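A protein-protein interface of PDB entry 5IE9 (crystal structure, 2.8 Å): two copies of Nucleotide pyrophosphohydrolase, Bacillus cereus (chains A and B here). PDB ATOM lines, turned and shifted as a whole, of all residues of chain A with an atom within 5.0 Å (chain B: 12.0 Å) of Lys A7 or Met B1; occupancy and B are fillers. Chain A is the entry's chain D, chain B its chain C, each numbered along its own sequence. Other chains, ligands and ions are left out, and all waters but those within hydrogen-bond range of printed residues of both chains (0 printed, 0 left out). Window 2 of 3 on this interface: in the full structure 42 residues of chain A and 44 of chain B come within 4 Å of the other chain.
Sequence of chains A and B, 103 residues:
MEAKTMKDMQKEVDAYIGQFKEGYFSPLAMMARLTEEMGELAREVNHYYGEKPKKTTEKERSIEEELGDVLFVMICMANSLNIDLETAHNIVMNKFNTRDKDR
The backbone NH (N) of Met A6 lies within hydrogen-bond range of the backbone carbonyl oxygen (O) of Lys B4, at 3.2 Å.
N of Lys B4 sits at hydrogen-bond distance from OE2 of Glu A86 (3.0 Å).
The side-chain carboxylate (OD2) of Asp B8 sits at hydrogen-bond distance from the side-chain hydroxyl (OG1) of Thr B5, 2.8 Å away.
The side-chain hydroxyl (OG1) of Thr A5 sits at hydrogen-bond distance from the side-chain carboxylate (OD2) of Asp A8 (2.9 Å).
NZ of Lys A7 lies within salt-bridge range of OD2 of Asp A84 (3.0 Å).
The side-chain carboxylate of Glu A86 is in salt-bridge range of the side-chain amino group of Lys A7, 2.9 Å away.
Among the printed residues, pairs that only touch across the chains: Thr A5 with Ala B3 (3.4 Å), Thr A5 with Lys B4 (3.4 Å), Thr A5 with Thr B5 (3.8 Å), Met A6 with Met B9 (3.99 Å), Lys A7 with Met B1 (3.8 Å), Met A9 with Met B6 (3.9 Å), Met A9 with His B89 (3.5 Å), Glu A86 with Glu B2 (3.6 Å) and Glu A86 with Ala B3 (3.9 Å).
Lys A7 touches just one residue of chain B: Met B1.
Of the printed residues of chain A, Met B1 touches Lys A7.
Thr A5 touches three residues of chain B.
No residue of chain B comes within 4 Å of Asp A8.
Met A9 touches just these residues of chain B: Met B6 (3.9 Å) and His B89 (3.5 Å).
No residue of chain B comes within 4 Å of Gln A10.
No residue of chain B comes within 4 Å of Asp A84.
Printed residues of chain B within 4 Å of Glu A86: Glu B2 (3.6 Å), Ala B3 (3.9 Å) and Lys B4 (3.0 Å).
Of the printed residues of chain A, Thr B5 touches Thr A5 (3.8 Å).
Of the printed residues of chain A, Met B6 touches Met A9 (3.9 Å).
Printed residues of chain A within 4 Å of Lys B4: Thr A5 (3.4 Å), Met A6 (3.2 Å) and Glu A86 (3.0 Å).
Of the printed residues of chain B, Met A6 touches Lys B4 (3.2 Å) and Met B9 (3.99 Å).
Met B93 touches none of the printed residues of chain A.
The nearest printed residue of chain A that does not touch Met B1 is Glu A86 (5.7 Å).
Hydrophobic or aromatic side chains of chain B that line the printed part of chain A: Met B1, Ala B3, Met B6, Met B9 and His B89.
Printed residues of chain A that touch a printed residue of chain B: Thr A5, Met A6, Lys A7, Met A9 and Glu A86.
Hydrophobic or aromatic side chains of chain A that line the printed part of chain B: Met A6 and Met A9.
Among the printed residues, no Asp or Glu carboxylate lies within 4 Å of a Lys or Arg side-chain nitrogen of the other chain.
Thr A5 touches its own counterpart, Thr B5.
Met A6 touches Met B9, and with the chains exchanged Met A9 touches Met B6.
6 positions are printed for both chains.
Of the 11 pairs that touch across the chains among the printed residues, 3 have their exchanged pair printed and touching as well.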
ATOM      1  N   THR A   5       2.700 -14.128  17.917  1.00  0.00           N
ATOM      2  CA  THR A   5       3.089 -15.380  18.566  1.00  0.00           C
ATOM      3  C   THR A   5       3.904 -15.080  19.815  1.00  0.00           C
ATOM      4  O   THR A   5       4.507 -14.009  19.918  1.00  0.00           O
ATOM      5  CB  THR A   5       3.911 -16.296  17.633  1.00  0.00           C
ATOM      6  OG1 THR A   5       5.063 -15.591  17.156  1.00  0.00           O
ATOM      7  CG2 THR A   5       3.070 -16.781  16.453  1.00  0.00           C
ATOM      8  N   MET A   6       3.922 -16.028  20.753  1.00  0.00           N
ATOM      9  CA  MET A   6       4.720 -15.911  21.979  1.00  0.00           C
ATOM     10  C   MET A   6       6.203 -15.699  21.661  1.00  0.00           C
ATOM     11  O   MET A   6       6.849 -14.848  22.279  1.00  0.00           O
ATOM     12  CB  MET A   6       4.514 -17.129  22.898  1.00  0.00           C
ATOM     13  CG  MET A   6       5.109 -16.982  24.294  1.00  0.00           C
ATOM     14  SD  MET A   6       4.283 -15.745  25.319  1.00  0.00           S
ATOM     15  CE  MET A   6       5.692 -14.813  25.881  1.00  0.00           C
ATOM     16  N   LYS A   7       6.713 -16.453  20.684  1.00  0.00           N
ATOM     17  CA  LYS A   7       8.099 -16.336  20.213  1.00  0.00           C
ATOM     18  C   LYS A   7       8.448 -14.924  19.744  1.00  0.00           C
ATOM     19  O   LYS A   7       9.532 -14.421  20.059  1.00  0.00           O
ATOM     20  CB  LYS A   7       8.395 -17.365  19.117  1.00  0.00           C
ATOM     21  CG  LYS A   7       8.721 -18.746  19.658  1.00  0.00           C
ATOM     22  CD  LYS A   7       8.979 -19.741  18.539  1.00  0.00           C
ATOM     23  CE  LYS A   7       9.490 -21.078  19.066  1.00  0.00           C
ATOM     24  NZ  LYS A   7       8.506 -21.800  19.923  1.00  0.00           N
ATOM     25  N   ASP A   8       7.517 -14.297  19.018  1.00  0.00           N
ATOM     26  CA  ASP A   8       7.651 -12.911  18.559  1.00  0.00           C
ATOM     27  C   ASP A   8       7.725 -11.912  19.713  1.00  0.00           C
ATOM     28  O   ASP A   8       8.605 -11.049  19.723  1.00  0.00           O
ATOM     29  CB  ASP A   8       6.506 -12.523  17.609  1.00  0.00           C
ATOM     30  CG  ASP A   8       6.657 -13.118  16.213  1.00  0.00           C
ATOM     31  OD1 ASP A   8       7.789 -13.467  15.801  1.00  0.00           O
ATOM     32  OD2 ASP A   8       5.623 -13.231  15.521  1.00  0.00           O
ATOM     33  N   MET A   9       6.811 -12.035  20.680  1.00  0.00           N
ATOM     34  CA  MET A   9       6.790 -11.163  21.863  1.00  0.00           C
ATOM     35  C   MET A   9       8.101 -11.257  22.639  1.00  0.00           C
ATOM     36  O   MET A   9       8.598 -10.245  23.128  1.00  0.00           O
ATOM     37  CB  MET A   9       5.612 -11.485  22.786  1.00  0.00           C
ATOM     38  CG  MET A   9       4.296 -11.764  22.077  1.00  0.00           C
ATOM     39  SD  MET A   9       2.768 -11.570  23.020  1.00  0.00           S
ATOM     40  CE  MET A   9       3.160 -12.247  24.632  1.00  0.00           C
ATOM     41  N   GLN A  10       8.655 -12.471  22.728  1.00  0.00           N
ATOM     42  CA  GLN A  10       9.969 -12.713  23.339  1.00  0.00           C
ATOM     43  C   GLN A  10      11.121 -12.094  22.536  1.00  0.00           C
ATOM     44  O   GLN A  10      11.989 -11.435  23.115  1.00  0.00           O
ATOM     45  CB  GLN A  10      10.208 -14.209  23.602  1.00  0.00           C
ATOM     46  CG  GLN A  10       9.253 -14.813  24.621  1.00  0.00           C
ATOM     47  CD  GLN A  10       9.654 -16.195  25.095  1.00  0.00           C
ATOM     48  OE1 GLN A  10       9.018 -17.191  24.745  1.00  0.00           O
ATOM     49  NE2 GLN A  10      10.700 -16.266  25.904  1.00  0.00           N
ATOM     50  N   LYS A  11      11.115 -12.299  21.213  1.00  0.00           N
ATOM     51  CA  LYS A  11      12.066 -11.648  20.290  1.00  0.00           C
ATOM     52  C   LYS A  11      12.023 -10.114  20.411  1.00  0.00           C
ATOM     53  O   LYS A  11      13.067  -9.453  20.421  1.00  0.00           O
ATOM     54  CB  LYS A  11      11.806 -12.080  18.833  1.00  0.00           C
ATOM     55  CG  LYS A  11      12.397 -13.435  18.449  1.00  0.00           C
ATOM     56  CD  LYS A  11      11.968 -13.887  17.053  1.00  0.00           C
ATOM     57  N   ASP A  84      11.956 -20.873  26.183  1.00  0.00           N
ATOM     58  CA  ASP A  84      10.821 -20.524  25.341  1.00  0.00           C
ATOM     59  C   ASP A  84       9.505 -20.780  26.065  1.00  0.00           C
ATOM     60  O   ASP A  84       9.172 -21.930  26.364  1.00  0.00           O
ATOM     61  CB  ASP A  84      10.861 -21.288  24.016  1.00  0.00           C
ATOM     62  CG  ASP A  84       9.618 -21.061  23.187  1.00  0.00           C
ATOM     63  OD1 ASP A  84       9.311 -19.892  22.843  1.00  0.00           O
ATOM     64  OD2 ASP A  84       8.933 -22.060  22.900  1.00  0.00           O
ATOM     65  N   GLU A  86       6.432 -20.708  25.056  1.00  0.00           N
ATOM     66  CA  GLU A  86       5.489 -21.568  24.345  1.00  0.00           C
ATOM     67  C   GLU A  86       5.685 -23.019  24.793  1.00  0.00           C
ATOM     68  O   GLU A  86       4.706 -23.707  25.096  1.00  0.00           O
ATOM     69  CB  GLU A  86       5.656 -21.429  22.828  1.00  0.00           C
ATOM     70  CG  GLU A  86       4.615 -22.167  21.983  1.00  0.00           C
ATOM     71  CD  GLU A  86       4.824 -22.012  20.477  1.00  0.00           C
ATOM     72  OE1 GLU A  86       5.632 -21.148  20.045  1.00  0.00           O
ATOM     73  OE2 GLU A  86       4.164 -22.757  19.716  1.00  0.00           O
ATOM     74  N   MET B   1       9.511 -22.728  14.435  1.00  0.00           N
ATOM     75  CA  MET B   1       8.322 -22.119  15.097  1.00  0.00           C
ATOM     76  C   MET B   1       7.021 -22.762  14.598  1.00  0.00           C
ATOM     77  O   MET B   1       6.805 -22.873  13.384  1.00  0.00           O
ATOM     78  CB  MET B   1       8.310 -20.604  14.868  1.00  0.00           C
ATOM     79  N   GLU B   2       6.177 -23.188  15.545  1.00  0.00           N
ATOM     80  CA  GLU B   2       4.888 -23.855  15.252  1.00  0.00           C
ATOM     81  C   GLU B   2       3.853 -23.008  14.462  1.00  0.00           C
ATOM     82  O   GLU B   2       3.437 -23.448  13.384  1.00  0.00           O
ATOM     83  CB  GLU B   2       4.276 -24.477  16.513  1.00  0.00           C
ATOM     84  N   ALA B   3       3.428 -21.823  14.936  1.00  0.00           N
ATOM     85  CA  ALA B   3       3.784 -21.183  16.218  1.00  0.00           C
ATOM     86  C   ALA B   3       2.535 -20.596  16.859  1.00  0.00           C
ATOM     87  O   ALA B   3       1.748 -19.922  16.185  1.00  0.00           O
ATOM     88  CB  ALA B   3       4.827 -20.084  16.016  1.00  0.00           C
ATOM     89  N   LYS B   4       2.369 -20.850  18.156  1.00  0.00           N
ATOM     90  CA  LYS B   4       1.167 -20.454  18.890  1.00  0.00           C
ATOM     91  C   LYS B   4       1.136 -18.971  19.210  1.00  0.00           C
ATOM     92  O   LYS B   4       2.122 -18.407  19.706  1.00  0.00           O
ATOM     93  CB  LYS B   4       1.027 -21.257  20.183  1.00  0.00           C
ATOM     94  CG  LYS B   4       0.501 -22.665  19.989  1.00  0.00           C
ATOM     95  CD  LYS B   4       0.003 -23.239  21.298  1.00  0.00           C
ATOM     96  CE  LYS B   4      -0.228 -24.730  21.170  1.00  0.00           C
ATOM     97  NZ  LYS B   4      -0.570 -25.318  22.489  1.00  0.00           N
ATOM     98  N   THR B   5      -0.006 -18.351  18.922  1.00  0.00           N
ATOM     99  CA  THR B   5      -0.261 -16.960  19.303  1.00  0.00           C
ATOM    100  C   THR B   5      -0.668 -16.887  20.770  1.00  0.00           C
ATOM    101  O   THR B   5      -1.201 -17.856  21.311  1.00  0.00           O
ATOM    102  CB  THR B   5      -1.385 -16.322  18.465  1.00  0.00           C
ATOM    103  OG1 THR B   5      -2.575 -17.101  18.598  1.00  0.00           O
ATOM    104  CG2 THR B   5      -0.997 -16.208  16.987  1.00  0.00           C
ATOM    105  N   MET B   6      -0.430 -15.731  21.393  1.00  0.00           N
ATOM    106  CA  MET B   6      -0.902 -15.436  22.755  1.00  0.00           C
ATOM    107  C   MET B   6      -2.427 -15.595  22.856  1.00  0.00           C
ATOM    108  O   MET B   6      -2.927 -16.126  23.849  1.00  0.00           O
ATOM    109  CB  MET B   6      -0.456 -14.027  23.185  1.00  0.00           C
ATOM    110  CG  MET B   6      -0.692 -13.647  24.643  1.00  0.00           C
ATOM    111  SD  MET B   6       0.291 -14.544  25.872  1.00  0.00           S
ATOM    112  CE  MET B   6      -0.932 -15.685  26.484  1.00  0.00           C
ATOM    113  N   LYS B   7      -3.145 -15.162  21.816  1.00  0.00           N
ATOM    114  CA  LYS B   7      -4.600 -15.315  21.733  1.00  0.00           C
ATOM    115  C   LYS B   7      -5.046 -16.770  21.830  1.00  0.00           C
ATOM    116  O   LYS B   7      -6.003 -17.070  22.548  1.00  0.00           O
ATOM    117  CB  LYS B   7      -5.156 -14.663  20.465  1.00  0.00           C
ATOM    118  CG  LYS B   7      -5.342 -13.164  20.597  1.00  0.00           C
ATOM    119  CD  LYS B   7      -6.445 -12.651  19.683  1.00  0.00           C
ATOM    120  CE  LYS B   7      -6.831 -11.212  20.012  1.00  0.00           C
ATOM    121  NZ  LYS B   7      -5.732 -10.228  19.795  1.00  0.00           N
ATOM    122  N   ASP B   8      -4.340 -17.660  21.126  1.00  0.00           N
ATOM    123  CA  ASP B   8      -4.615 -19.103  21.162  1.00  0.00           C
ATOM    124  C   ASP B   8      -4.307 -19.752  22.516  1.00  0.00           C
ATOM    125  O   ASP B   8      -5.103 -20.559  23.000  1.00  0.00           O
ATOM    126  CB  ASP B   8      -3.875 -19.842  20.040  1.00  0.00           C
ATOM    127  CG  ASP B   8      -4.433 -19.534  18.656  1.00  0.00           C
ATOM    128  OD1 ASP B   8      -5.662 -19.339  18.507  1.00  0.00           O
ATOM    129  OD2 ASP B   8      -3.622 -19.492  17.707  1.00  0.00           O
ATOM    130  N   MET B   9      -3.167 -19.402  23.121  1.00  0.00           N
ATOM    131  CA  MET B   9      -2.791 -19.902  24.456  1.00  0.00           C
ATOM    132  C   MET B   9      -3.860 -19.542  25.489  1.00  0.00           C
ATOM    133  O   MET B   9      -4.179 -20.355  26.355  1.00  0.00           O
ATOM    134  CB  MET B   9      -1.428 -19.365  24.908  1.00  0.00           C
ATOM    135  CG  MET B   9      -0.361 -19.301  23.827  1.00  0.00           C
ATOM    136  SD  MET B   9       1.389 -19.293  24.288  1.00  0.00           S
ATOM    137  CE  MET B   9       1.434 -18.476  25.881  1.00  0.00           C
ATOM    138  N   GLU B  64      11.970 -23.944  33.961  1.00  0.00           N
ATOM    139  CA  GLU B  64      11.111 -23.810  32.783  1.00  0.00           C
ATOM    140  C   GLU B  64       9.647 -24.100  33.125  1.00  0.00           C
ATOM    141  O   GLU B  64       8.755 -23.354  32.717  1.00  0.00           O
ATOM    142  CB  GLU B  64      11.605 -24.734  31.661  1.00  0.00           C
ATOM    143  CG  GLU B  64      10.783 -24.709  30.375  1.00  0.00           C
ATOM    144  CD  GLU B  64      11.153 -25.819  29.401  1.00  0.00           C
ATOM    145  OE1 GLU B  64      11.346 -26.981  29.831  1.00  0.00           O
ATOM    146  OE2 GLU B  64      11.238 -25.532  28.189  1.00  0.00           O
ATOM    147  N   LEU B  71       2.749 -18.496  34.371  1.00  0.00           N
ATOM    148  CA  LEU B  71       2.103 -18.054  33.137  1.00  0.00           C
ATOM    149  C   LEU B  71       0.654 -18.537  33.031  1.00  0.00           C
ATOM    150  O   LEU B  71      -0.205 -17.815  32.528  1.00  0.00           O
ATOM    151  CB  LEU B  71       2.903 -18.539  31.923  1.00  0.00           C
ATOM    152  CG  LEU B  71       3.032 -17.779  30.585  1.00  0.00           C
ATOM    153  CD1 LEU B  71       2.881 -18.792  29.464  1.00  0.00           C
ATOM    154  CD2 LEU B  71       2.072 -16.615  30.357  1.00  0.00           C
ATOM    155  N   ILE B  75      -2.681 -16.215  32.737  1.00  0.00           N
ATOM    156  CA  ILE B  75      -3.649 -16.372  31.657  1.00  0.00           C
ATOM    157  C   ILE B  75      -5.051 -16.501  32.252  1.00  0.00           C
ATOM    158  O   ILE B  75      -5.980 -15.836  31.794  1.00  0.00           O
ATOM    159  CB  ILE B  75      -3.286 -17.534  30.697  1.00  0.00           C
ATOM    160  CG1 ILE B  75      -2.066 -17.152  29.847  1.00  0.00           C
ATOM    161  CG2 ILE B  75      -4.456 -17.852  29.774  1.00  0.00           C
ATOM    162  CD1 ILE B  75      -1.380 -18.302  29.134  1.00  0.00           C
ATOM    163  N   LEU B  85      -3.777 -10.455  26.708  1.00  0.00           N
ATOM    164  CA  LEU B  85      -2.358 -10.247  27.070  1.00  0.00           C
ATOM    165  C   LEU B  85      -1.453  -9.759  25.924  1.00  0.00           C
ATOM    166  O   LEU B  85      -0.356  -9.255  26.180  1.00  0.00           O
ATOM    167  CB  LEU B  85      -1.753 -11.495  27.729  1.00  0.00           C
ATOM    168  CG  LEU B  85      -2.236 -11.931  29.113  1.00  0.00           C
ATOM    169  CD1 LEU B  85      -1.763 -13.347  29.388  1.00  0.00           C
ATOM    170  CD2 LEU B  85      -1.793 -11.000  30.236  1.00  0.00           C
ATOM    171  N   GLU B  86      -1.904  -9.920  24.679  1.00  0.00           N
ATOM    172  CA  GLU B  86      -1.225  -9.342  23.520  1.00  0.00           C
ATOM    173  C   GLU B  86      -1.351  -7.820  23.566  1.00  0.00           C
ATOM    174  O   GLU B  86      -0.358  -7.111  23.372  1.00  0.00           O
ATOM    175  CB  GLU B  86      -1.795  -9.901  22.213  1.00  0.00           C
ATOM    176  CG  GLU B  86      -1.048  -9.473  20.950  1.00  0.00           C
ATOM    177  CD  GLU B  86      -1.657 -10.011  19.657  1.00  0.00           C
ATOM    178  OE1 GLU B  86      -2.574 -10.870  19.706  1.00  0.00           O
ATOM    179  OE2 GLU B  86      -1.204  -9.573  18.576  1.00  0.00           O
ATOM    180  N   HIS B  89       0.789  -6.534  26.535  1.00  0.00           N
ATOM    181  CA  HIS B  89       2.196  -6.531  26.119  1.00  0.00           C
ATOM    182  C   HIS B  89       2.527  -5.294  25.282  1.00  0.00           C
ATOM    183  O   HIS B  89       3.558  -4.652  25.503  1.00  0.00           O
ATOM    184  CB  HIS B  89       2.497  -7.823  25.346  1.00  0.00           C
ATOM    185  CG  HIS B  89       3.872  -7.886  24.757  1.00  0.00           C
ATOM    186  ND1 HIS B  89       4.136  -7.541  23.448  1.00  0.00           N
ATOM    187  CD2 HIS B  89       5.054  -8.277  25.287  1.00  0.00           C
ATOM    188  CE1 HIS B  89       5.424  -7.704  23.201  1.00  0.00           C
ATOM    189  NE2 HIS B  89       6.002  -8.153  24.300  1.00  0.00           N
ATOM    190  N   ASN B  90       1.634  -4.971  24.342  1.00  0.00           N
ATOM    191  CA  ASN B  90       1.784  -3.834  23.435  1.00  0.00           C
ATOM    192  C   ASN B  90       1.800  -2.486  24.127  1.00  0.00           C
ATOM    193  O   ASN B  90       2.567  -1.606  23.719  1.00  0.00           O
ATOM    194  CB  ASN B  90       0.696  -3.835  22.354  1.00  0.00           C
ATOM    195  CG  ASN B  90       0.924  -4.904  21.284  1.00  0.00           C
ATOM    196  OD1 ASN B  90       2.054  -5.338  21.040  1.00  0.00           O
ATOM    197  ND2 ASN B  90      -0.154  -5.314  20.628  1.00  0.00           N
ATOM    198  N   MET B  93       5.221  -2.190  25.768  1.00  0.00           N
ATOM    199  CA  MET B  93       6.196  -1.936  24.704  1.00  0.00           C
ATOM    200  C   MET B  93       6.136  -0.513  24.148  1.00  0.00           C
ATOM    201  O   MET B  93       7.170   0.057  23.804  1.00  0.00           O
ATOM    202  CB  MET B  93       6.055  -2.970  23.583  1.00  0.00           C
ATOM    203  CG  MET B  93       6.558  -4.369  23.933  1.00  0.00           C
ATOM    204  SD  MET B  93       8.338  -4.493  24.246  1.00  0.00           S
ATOM    205  CE  MET B  93       8.329  -4.459  26.027  1.00  0.00           C
